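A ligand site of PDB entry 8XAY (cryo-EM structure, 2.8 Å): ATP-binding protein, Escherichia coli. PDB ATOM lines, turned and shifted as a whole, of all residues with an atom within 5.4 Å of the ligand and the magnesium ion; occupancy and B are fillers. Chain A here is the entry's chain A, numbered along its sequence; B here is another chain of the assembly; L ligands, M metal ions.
NH2 of Arg 455 of chain B sits close to S1 of the ligand (2.8 Å).
S1 of the ligand sits close to NZ of Lys 456 of chain B (3.3 Å).
The backbone NH (N) of Gly 156 sits at hydrogen-bond distance from an oxygen (O3) of the ligand, at 2.7 Å.
An oxygen (O6) of the ligand is in hydrogen-bond range of the backbone NH of His 159 (3.2 Å).
An oxygen (O5) of the ligand is in hydrogen-bond range of the backbone NH (N) of Gly 154, 2.8 Å away.
N of Lys 157 is in hydrogen-bond range of O3 of the ligand (2.5 Å).
O3 of the ligand is in salt-bridge range of NZ of Lys 157, at 3.7 Å.
N of Ser 158 lies within hydrogen-bond range of O6 of the ligand (3.0 Å).
The backbone carbonyl oxygen (O) of Ile 534 is in hydrogen-bond range of a nitrogen (N3) of the ligand (2.8 Å).
The backbone NH (N) of Ser 155 lies within hydrogen-bond range of an oxygen (O3) of the ligand (3.4 Å).
The side-chain carboxylate of Glu 426 sits close to the side-chain hydroxyl of Ser 158.
OG1 of Thr 160 sits at hydrogen-bond distance from O of Gly 156.
O of Gly 517 sits at hydrogen-bond distance from N of Ile 534.
NZ of Lys 157 sits at hydrogen-bond distance from O of Ser 152.
The side-chain hydroxyl (OG) of Ser 155 lies within hydrogen-bond range of the backbone carbonyl oxygen (O) of Ser 152 (2.7 Å).
OG of Ser 158 lies close to OE2 of Glu 192 (3.0 Å).
The backbone NH (N) of Gly 517 is in hydrogen-bond range of the backbone carbonyl oxygen (O) of Ser 155.
The side-chain carboxylate (OE2) of Glu 516 lies close to an oxygen (O10) of the ligand (3.4 Å).
Thr 153 touches the ligand (CA to O2, 3.8 Å).
Gly 517 touches the ligand (CA to C8, 3.5 Å).
Lys 536 touches the ligand (CG to N4, 3.4 Å).
Hydrophobic or aromatic side chains that line the ligand: His 159.
Two residues have an atom within 4 Å of the magnesium ion: Ser 158 and Glu 192.
The magnesium ion is bound by O1 of the ligand, OG of Ser 158 and O4 of the ligand.
Slightly farther from the magnesium ion lies the side-chain carboxylate (OE2) of Glu 192 (2.7 Å).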
ATOM      1  N   SER A 152     -22.217  -8.720 -23.081  1.00  0.00           N
ATOM      2  CA  SER A 152     -21.838  -7.934 -21.913  1.00  0.00           C
ATOM      3  C   SER A 152     -20.350  -8.109 -21.629  1.00  0.00           C
ATOM      4  O   SER A 152     -19.646  -8.839 -22.330  1.00  0.00           O
ATOM      5  CB  SER A 152     -22.686  -8.314 -20.710  1.00  0.00           C
ATOM      6  OG  SER A 152     -22.150  -9.441 -20.046  1.00  0.00           O
ATOM      7  N   THR A 153     -19.869  -7.427 -20.601  1.00  0.00           N
ATOM      8  CA  THR A 153     -18.466  -7.547 -20.212  1.00  0.00           C
ATOM      9  C   THR A 153     -18.210  -8.911 -19.608  1.00  0.00           C
ATOM     10  O   THR A 153     -18.947  -9.367 -18.726  1.00  0.00           O
ATOM     11  CB  THR A 153     -18.093  -6.447 -19.227  1.00  0.00           C
ATOM     12  OG1 THR A 153     -18.761  -6.673 -17.972  1.00  0.00           O
ATOM     13  CG2 THR A 153     -18.495  -5.088 -19.771  1.00  0.00           C
ATOM     14  N   GLY A 154     -17.160  -9.572 -20.069  1.00  0.00           N
ATOM     15  CA  GLY A 154     -16.841 -10.906 -19.596  1.00  0.00           C
ATOM     16  C   GLY A 154     -17.697 -12.016 -20.165  1.00  0.00           C
ATOM     17  O   GLY A 154     -17.603 -13.151 -19.685  1.00  0.00           O
ATOM     18  N   SER A 155     -18.519 -11.726 -21.168  1.00  0.00           N
ATOM     19  CA  SER A 155     -19.399 -12.752 -21.726  1.00  0.00           C
ATOM     20  C   SER A 155     -18.624 -13.773 -22.551  1.00  0.00           C
ATOM     21  O   SER A 155     -19.032 -14.931 -22.651  1.00  0.00           O
ATOM     22  CB  SER A 155     -20.485 -12.101 -22.579  1.00  0.00           C
ATOM     23  OG  SER A 155     -19.926 -11.225 -23.538  1.00  0.00           O
ATOM     24  N   GLY A 156     -17.509 -13.364 -23.166  1.00  0.00           N
ATOM     25  CA  GLY A 156     -16.711 -14.285 -23.943  1.00  0.00           C
ATOM     26  C   GLY A 156     -16.421 -13.793 -25.337  1.00  0.00           C
ATOM     27  O   GLY A 156     -16.058 -14.577 -26.221  1.00  0.00           O
ATOM     28  N   LYS A 157     -16.611 -12.487 -25.561  1.00  0.00           N
ATOM     29  CA  LYS A 157     -16.499 -11.902 -26.897  1.00  0.00           C
ATOM     30  C   LYS A 157     -15.092 -12.050 -27.456  1.00  0.00           C
ATOM     31  O   LYS A 157     -14.908 -12.446 -28.605  1.00  0.00           O
ATOM     32  CB  LYS A 157     -16.873 -10.429 -26.843  1.00  0.00           C
ATOM     33  CG  LYS A 157     -18.359 -10.150 -26.744  1.00  0.00           C
ATOM     34  CD  LYS A 157     -18.659  -8.755 -27.222  1.00  0.00           C
ATOM     35  CE  LYS A 157     -17.919  -7.684 -26.427  1.00  0.00           C
ATOM     36  NZ  LYS A 157     -17.817  -7.962 -24.956  1.00  0.00           N
ATOM     37  N   SER A 158     -14.078 -11.715 -26.652  1.00  0.00           N
ATOM     38  CA  SER A 158     -12.704 -11.763 -27.125  1.00  0.00           C
ATOM     39  C   SER A 158     -12.230 -13.195 -27.350  1.00  0.00           C
ATOM     40  O   SER A 158     -11.428 -13.449 -28.252  1.00  0.00           O
ATOM     41  CB  SER A 158     -11.774 -11.049 -26.145  1.00  0.00           C
ATOM     42  OG  SER A 158     -12.166  -9.695 -25.984  1.00  0.00           O
ATOM     43  N   HIS A 159     -12.705 -14.139 -26.538  1.00  0.00           N
ATOM     44  CA  HIS A 159     -12.410 -15.541 -26.793  1.00  0.00           C
ATOM     45  C   HIS A 159     -13.141 -16.033 -28.028  1.00  0.00           C
ATOM     46  O   HIS A 159     -12.613 -16.866 -28.774  1.00  0.00           O
ATOM     47  CB  HIS A 159     -12.781 -16.382 -25.571  1.00  0.00           C
ATOM     48  CG  HIS A 159     -11.740 -16.400 -24.496  1.00  0.00           C
ATOM     49  ND1 HIS A 159     -11.080 -15.265 -24.092  1.00  0.00           N
ATOM     50  CD2 HIS A 159     -11.252 -17.420 -23.759  1.00  0.00           C
ATOM     51  CE1 HIS A 159     -10.223 -15.580 -23.131  1.00  0.00           C
ATOM     52  NE2 HIS A 159     -10.310 -16.882 -22.915  1.00  0.00           N
ATOM     53  N   THR A 160     -14.365 -15.548 -28.258  1.00  0.00           N
ATOM     54  CA  THR A 160     -15.098 -15.869 -29.477  1.00  0.00           C
ATOM     55  C   THR A 160     -14.393 -15.319 -30.707  1.00  0.00           C
ATOM     56  O   THR A 160     -14.250 -16.022 -31.713  1.00  0.00           O
ATOM     57  CB  THR A 160     -16.517 -15.325 -29.389  1.00  0.00           C
ATOM     58  OG1 THR A 160     -17.183 -15.940 -28.279  1.00  0.00           O
ATOM     59  CG2 THR A 160     -17.292 -15.595 -30.662  1.00  0.00           C
ATOM     60  N   HIS A 190      -6.785  -3.282 -26.293  1.00  0.00           N
ATOM     61  CA  HIS A 190      -6.376  -3.681 -24.954  1.00  0.00           C
ATOM     62  C   HIS A 190      -5.079  -4.476 -24.949  1.00  0.00           C
ATOM     63  O   HIS A 190      -4.671  -4.957 -23.880  1.00  0.00           O
ATOM     64  CB  HIS A 190      -7.489  -4.477 -24.278  1.00  0.00           C
ATOM     65  CG  HIS A 190      -8.711  -3.665 -23.973  1.00  0.00           C
ATOM     66  ND1 HIS A 190      -8.649  -2.460 -23.325  1.00  0.00           N
ATOM     67  CD2 HIS A 190     -10.019  -3.893 -24.242  1.00  0.00           C
ATOM     68  CE1 HIS A 190      -9.868  -1.969 -23.195  1.00  0.00           C
ATOM     69  NE2 HIS A 190     -10.720  -2.820 -23.738  1.00  0.00           N
ATOM     70  N   GLU A 192      -4.347  -7.445 -26.199  1.00  0.00           N
ATOM     71  CA  GLU A 192      -4.753  -8.714 -25.630  1.00  0.00           C
ATOM     72  C   GLU A 192      -4.740  -9.886 -26.612  1.00  0.00           C
ATOM     73  O   GLU A 192      -4.771 -11.040 -26.156  1.00  0.00           O
ATOM     74  CB  GLU A 192      -6.156  -8.593 -25.026  1.00  0.00           C
ATOM     75  CG  GLU A 192      -7.247  -8.382 -26.045  1.00  0.00           C
ATOM     76  CD  GLU A 192      -8.546  -9.061 -25.665  1.00  0.00           C
ATOM     77  OE1 GLU A 192      -8.558 -10.299 -25.558  1.00  0.00           O
ATOM     78  OE2 GLU A 192      -9.550  -8.350 -25.472  1.00  0.00           O
ATOM     79  N   TYR A 193      -4.684  -9.641 -27.908  1.00  0.00           N
ATOM     80  CA  TYR A 193      -4.728 -10.710 -28.894  1.00  0.00           C
ATOM     81  C   TYR A 193      -3.351 -11.248 -29.265  1.00  0.00           C
ATOM     82  O   TYR A 193      -3.260 -12.134 -30.125  1.00  0.00           O
ATOM     83  CB  TYR A 193      -5.455 -10.251 -30.156  1.00  0.00           C
ATOM     84  CG  TYR A 193      -6.948 -10.113 -29.994  1.00  0.00           C
ATOM     85  CD1 TYR A 193      -7.769 -11.230 -30.012  1.00  0.00           C
ATOM     86  CD2 TYR A 193      -7.534  -8.866 -29.805  1.00  0.00           C
ATOM     87  CE1 TYR A 193      -9.137 -11.117 -29.849  1.00  0.00           C
ATOM     88  CE2 TYR A 193      -8.896  -8.745 -29.645  1.00  0.00           C
ATOM     89  CZ  TYR A 193      -9.689  -9.871 -29.669  1.00  0.00           C
ATOM     90  OH  TYR A 193     -11.048  -9.755 -29.517  1.00  0.00           O
ATOM     91  N   GLU A 426     -12.446  -4.277 -32.185  1.00  0.00           N
ATOM     92  CA  GLU A 426     -12.812  -4.435 -30.788  1.00  0.00           C
ATOM     93  C   GLU A 426     -13.233  -3.078 -30.230  1.00  0.00           C
ATOM     94  O   GLU A 426     -12.607  -2.055 -30.517  1.00  0.00           O
ATOM     95  CB  GLU A 426     -11.645  -4.993 -29.983  1.00  0.00           C
ATOM     96  CG  GLU A 426     -11.719  -6.502 -29.753  1.00  0.00           C
ATOM     97  CD  GLU A 426     -12.806  -6.909 -28.778  1.00  0.00           C
ATOM     98  OE1 GLU A 426     -13.264  -6.063 -27.993  1.00  0.00           O
ATOM     99  OE2 GLU A 426     -13.202  -8.091 -28.804  1.00  0.00           O
ATOM    100  N   GLN A 466     -18.912  -4.295 -26.432  1.00  0.00           N
ATOM    101  CA  GLN A 466     -19.625  -4.653 -25.216  1.00  0.00           C
ATOM    102  C   GLN A 466     -20.880  -3.818 -24.993  1.00  0.00           C
ATOM    103  O   GLN A 466     -21.738  -4.215 -24.197  1.00  0.00           O
ATOM    104  CB  GLN A 466     -18.698  -4.535 -24.001  1.00  0.00           C
ATOM    105  CG  GLN A 466     -18.198  -3.134 -23.720  1.00  0.00           C
ATOM    106  CD  GLN A 466     -16.766  -2.924 -24.166  1.00  0.00           C
ATOM    107  OE1 GLN A 466     -16.449  -3.056 -25.345  1.00  0.00           O
ATOM    108  NE2 GLN A 466     -15.897  -2.584 -23.228  1.00  0.00           N
ATOM    109  N   GLU A 516     -21.421 -18.247 -19.747  1.00  0.00           N
ATOM    110  CA  GLU A 516     -20.131 -17.756 -20.226  1.00  0.00           C
ATOM    111  C   GLU A 516     -19.706 -18.573 -21.447  1.00  0.00           C
ATOM    112  O   GLU A 516     -19.610 -19.799 -21.384  1.00  0.00           O
ATOM    113  CB  GLU A 516     -19.095 -17.849 -19.118  1.00  0.00           C
ATOM    114  CG  GLU A 516     -17.913 -16.922 -19.291  1.00  0.00           C
ATOM    115  CD  GLU A 516     -17.388 -16.417 -17.958  1.00  0.00           C
ATOM    116  OE1 GLU A 516     -17.519 -17.142 -16.954  1.00  0.00           O
ATOM    117  OE2 GLU A 516     -16.853 -15.292 -17.917  1.00  0.00           O
ATOM    118  N   GLY A 517     -19.450 -17.883 -22.562  1.00  0.00           N
ATOM    119  CA  GLY A 517     -19.148 -18.546 -23.813  1.00  0.00           C
ATOM    120  C   GLY A 517     -20.362 -19.020 -24.585  1.00  0.00           C
ATOM    121  O   GLY A 517     -20.189 -19.624 -25.655  1.00  0.00           O
ATOM    122  N   ILE A 534     -19.729 -22.081 -27.682  1.00  0.00           N
ATOM    123  CA  ILE A 534     -18.522 -21.957 -28.478  1.00  0.00           C
ATOM    124  C   ILE A 534     -17.383 -22.699 -27.798  1.00  0.00           C
ATOM    125  O   ILE A 534     -17.213 -22.622 -26.578  1.00  0.00           O
ATOM    126  CB  ILE A 534     -18.184 -20.468 -28.694  1.00  0.00           C
ATOM    127  CG1 ILE A 534     -19.408 -19.745 -29.261  1.00  0.00           C
ATOM    128  CG2 ILE A 534     -17.001 -20.289 -29.615  1.00  0.00           C
ATOM    129  CD1 ILE A 534     -19.309 -18.283 -29.176  1.00  0.00           C
ATOM    130  N   GLU A 535     -16.621 -23.450 -28.600  1.00  0.00           N
ATOM    131  CA  GLU A 535     -15.538 -24.257 -28.059  1.00  0.00           C
ATOM    132  C   GLU A 535     -14.451 -23.368 -27.466  1.00  0.00           C
ATOM    133  O   GLU A 535     -14.196 -22.257 -27.953  1.00  0.00           O
ATOM    134  CB  GLU A 535     -14.950 -25.161 -29.143  1.00  0.00           C
ATOM    135  CG  GLU A 535     -14.450 -24.442 -30.377  1.00  0.00           C
ATOM    136  CD  GLU A 535     -13.811 -25.380 -31.375  1.00  0.00           C
ATOM    137  OE1 GLU A 535     -12.749 -25.952 -31.063  1.00  0.00           O
ATOM    138  OE2 GLU A 535     -14.377 -25.556 -32.478  1.00  0.00           O
ATOM    139  N   LYS A 536     -13.848 -23.844 -26.382  1.00  0.00           N
ATOM    140  CA  LYS A 536     -12.909 -23.036 -25.614  1.00  0.00           C
ATOM    141  C   LYS A 536     -11.630 -22.797 -26.400  1.00  0.00           C
ATOM    142  O   LYS A 536     -11.223 -23.601 -27.249  1.00  0.00           O
ATOM    143  CB  LYS A 536     -12.592 -23.716 -24.291  1.00  0.00           C
ATOM    144  CG  LYS A 536     -13.696 -23.609 -23.248  1.00  0.00           C
ATOM    145  CD  LYS A 536     -13.310 -24.247 -21.919  1.00  0.00           C
ATOM    146  CE  LYS A 536     -11.876 -23.930 -21.517  1.00  0.00           C
ATOM    147  NZ  LYS A 536     -11.657 -22.473 -21.293  1.00  0.00           N
ATOM    148  N   PRO A 541      -6.691 -15.421 -25.464  1.00  0.00           N
ATOM    149  CA  PRO A 541      -6.133 -14.063 -25.435  1.00  0.00           C
ATOM    150  C   PRO A 541      -5.860 -13.615 -24.007  1.00  0.00           C
ATOM    151  O   PRO A 541      -6.371 -14.194 -23.038  1.00  0.00           O
ATOM    152  CB  PRO A 541      -7.241 -13.218 -26.077  1.00  0.00           C
ATOM    153  CG  PRO A 541      -8.469 -14.089 -25.951  1.00  0.00           C
ATOM    154  CD  PRO A 541      -7.925 -15.433 -26.264  1.00  0.00           C
ATOM    155  N   SER A 543      -6.296 -12.068 -20.766  1.00  0.00           N
ATOM    156  CA  SER A 543      -7.519 -11.724 -20.051  1.00  0.00           C
ATOM    157  C   SER A 543      -7.197 -10.812 -18.891  1.00  0.00           C
ATOM    158  O   SER A 543      -6.357 -11.149 -18.041  1.00  0.00           O
ATOM    159  CB  SER A 543      -8.235 -12.984 -19.550  1.00  0.00           C
ATOM    160  OG  SER A 543      -7.704 -13.381 -18.295  1.00  0.00           O
ATOM    161  N   ILE A 544      -7.853  -9.659 -18.842  1.00  0.00           N
ATOM    162  CA  ILE A 544      -7.656  -8.689 -17.781  1.00  0.00           C
ATOM    163  C   ILE A 544      -8.832  -8.857 -16.811  1.00  0.00           C
ATOM    164  O   ILE A 544      -9.905  -8.279 -17.003  1.00  0.00           O
ATOM    165  CB  ILE A 544      -7.565  -7.262 -18.322  1.00  0.00           C
ATOM    166  CG1 ILE A 544      -6.498  -7.171 -19.424  1.00  0.00           C
ATOM    167  CG2 ILE A 544      -7.308  -6.275 -17.191  1.00  0.00           C
ATOM    168  CD1 ILE A 544      -5.134  -7.743 -19.029  1.00  0.00           C
ATOM    169  N   ARG B 455     -12.270  -0.341 -15.273  1.00  0.00           N
ATOM    170  CA  ARG B 455     -12.279  -1.725 -14.810  1.00  0.00           C
ATOM    171  C   ARG B 455     -10.965  -2.433 -15.100  1.00  0.00           C
ATOM    172  O   ARG B 455     -10.487  -3.233 -14.291  1.00  0.00           O
ATOM    173  CB  ARG B 455     -13.450  -2.467 -15.451  1.00  0.00           C
ATOM    174  CG  ARG B 455     -13.643  -3.874 -14.959  1.00  0.00           C
ATOM    175  CD  ARG B 455     -14.973  -4.432 -15.410  1.00  0.00           C
ATOM    176  NE  ARG B 455     -14.939  -4.849 -16.812  1.00  0.00           N
ATOM    177  CZ  ARG B 455     -14.490  -6.027 -17.215  1.00  0.00           C
ATOM    178  NH1 ARG B 455     -14.053  -6.938 -16.367  1.00  0.00           N
ATOM    179  NH2 ARG B 455     -14.479  -6.297 -18.518  1.00  0.00           N
ATOM    180  N   LYS B 456     -10.372  -2.149 -16.262  1.00  0.00           N
ATOM    181  CA  LYS B 456      -9.169  -2.867 -16.676  1.00  0.00           C
ATOM    182  C   LYS B 456      -7.935  -2.441 -15.889  1.00  0.00           C
ATOM    183  O   LYS B 456      -7.063  -3.266 -15.607  1.00  0.00           O
ATOM    184  CB  LYS B 456      -8.941  -2.680 -18.172  1.00  0.00           C
ATOM    185  CG  LYS B 456     -10.203  -2.850 -19.012  1.00  0.00           C
ATOM    186  CD  LYS B 456     -10.550  -4.318 -19.201  1.00  0.00           C
ATOM    187  CE  LYS B 456     -11.016  -4.612 -20.618  1.00  0.00           C
ATOM    188  NZ  LYS B 456     -10.750  -6.016 -21.027  1.00  0.00           N
HETATM  189  P1  LIG L   1     -14.573  -7.738 -22.229  1.00  0.00           P
HETATM  190  S1  LIG L   1     -13.497  -7.868 -20.612  1.00  0.00           S
HETATM  191  O1  LIG L   1     -13.655  -7.701 -23.483  1.00  0.00           O
HETATM  192  O2  LIG L   1     -15.419  -6.436 -22.177  1.00  0.00           O
HETATM  193  P2  LIG L   1     -15.070 -10.300 -23.027  1.00  0.00           P
HETATM  194  O3  LIG L   1     -16.241 -11.037 -23.529  1.00  0.00           O
HETATM  195  O4  LIG L   1     -14.111  -9.867 -24.134  1.00  0.00           O
HETATM  196  O5  LIG L   1     -15.526  -8.967 -22.302  1.00  0.00           O
HETATM  197  P3  LIG L   1     -13.432 -12.457 -22.507  1.00  0.00           P
HETATM  198  O6  LIG L   1     -13.785 -12.821 -23.887  1.00  0.00           O
HETATM  199  O7  LIG L   1     -11.942 -12.159 -22.324  1.00  0.00           O
HETATM  200  O8  LIG L   1     -14.215 -11.181 -22.020  1.00  0.00           O
HETATM  201  O9  LIG L   1     -13.887 -13.621 -21.541  1.00  0.00           O
HETATM  202  C1  LIG L   1     -13.371 -13.704 -20.202  1.00  0.00           C
HETATM  203  C2  LIG L   1     -13.478 -15.126 -19.724  1.00  0.00           C
HETATM  204  O10 LIG L   1     -14.595 -15.764 -20.354  1.00  0.00           O
HETATM  205  C3  LIG L   1     -12.298 -16.032 -20.065  1.00  0.00           C
HETATM  206  O11 LIG L   1     -11.248 -15.893 -19.114  1.00  0.00           O
HETATM  207  C4  LIG L   1     -12.926 -17.429 -20.012  1.00  0.00           C
HETATM  208  O12 LIG L   1     -12.801 -18.004 -18.710  1.00  0.00           O
HETATM  209  C5  LIG L   1     -14.404 -17.161 -20.340  1.00  0.00           C
HETATM  210  N1  LIG L   1     -14.830 -17.704 -21.612  1.00  0.00           N
HETATM  211  C6  LIG L   1     -14.874 -17.057 -22.820  1.00  0.00           C
HETATM  212  N2  LIG L   1     -15.314 -17.797 -23.815  1.00  0.00           N
HETATM  213  C7  LIG L   1     -15.570 -19.027 -23.224  1.00  0.00           C
HETATM  214  C8  LIG L   1     -16.050 -20.246 -23.732  1.00  0.00           C
HETATM  215  N3  LIG L   1     -16.366 -20.430 -25.018  1.00  0.00           N
HETATM  216  N4  LIG L   1     -16.193 -21.272 -22.872  1.00  0.00           N
HETATM  217  C9  LIG L   1     -15.878 -21.089 -21.586  1.00  0.00           C
HETATM  218  N5  LIG L   1     -15.410 -19.987 -20.994  1.00  0.00           N
HETATM  219  C10 LIG L   1     -15.278 -18.984 -21.871  1.00  0.00           C
HETATM  220 MG    MG M   1     -12.010  -8.422 -24.404  1.00  0.00          MG
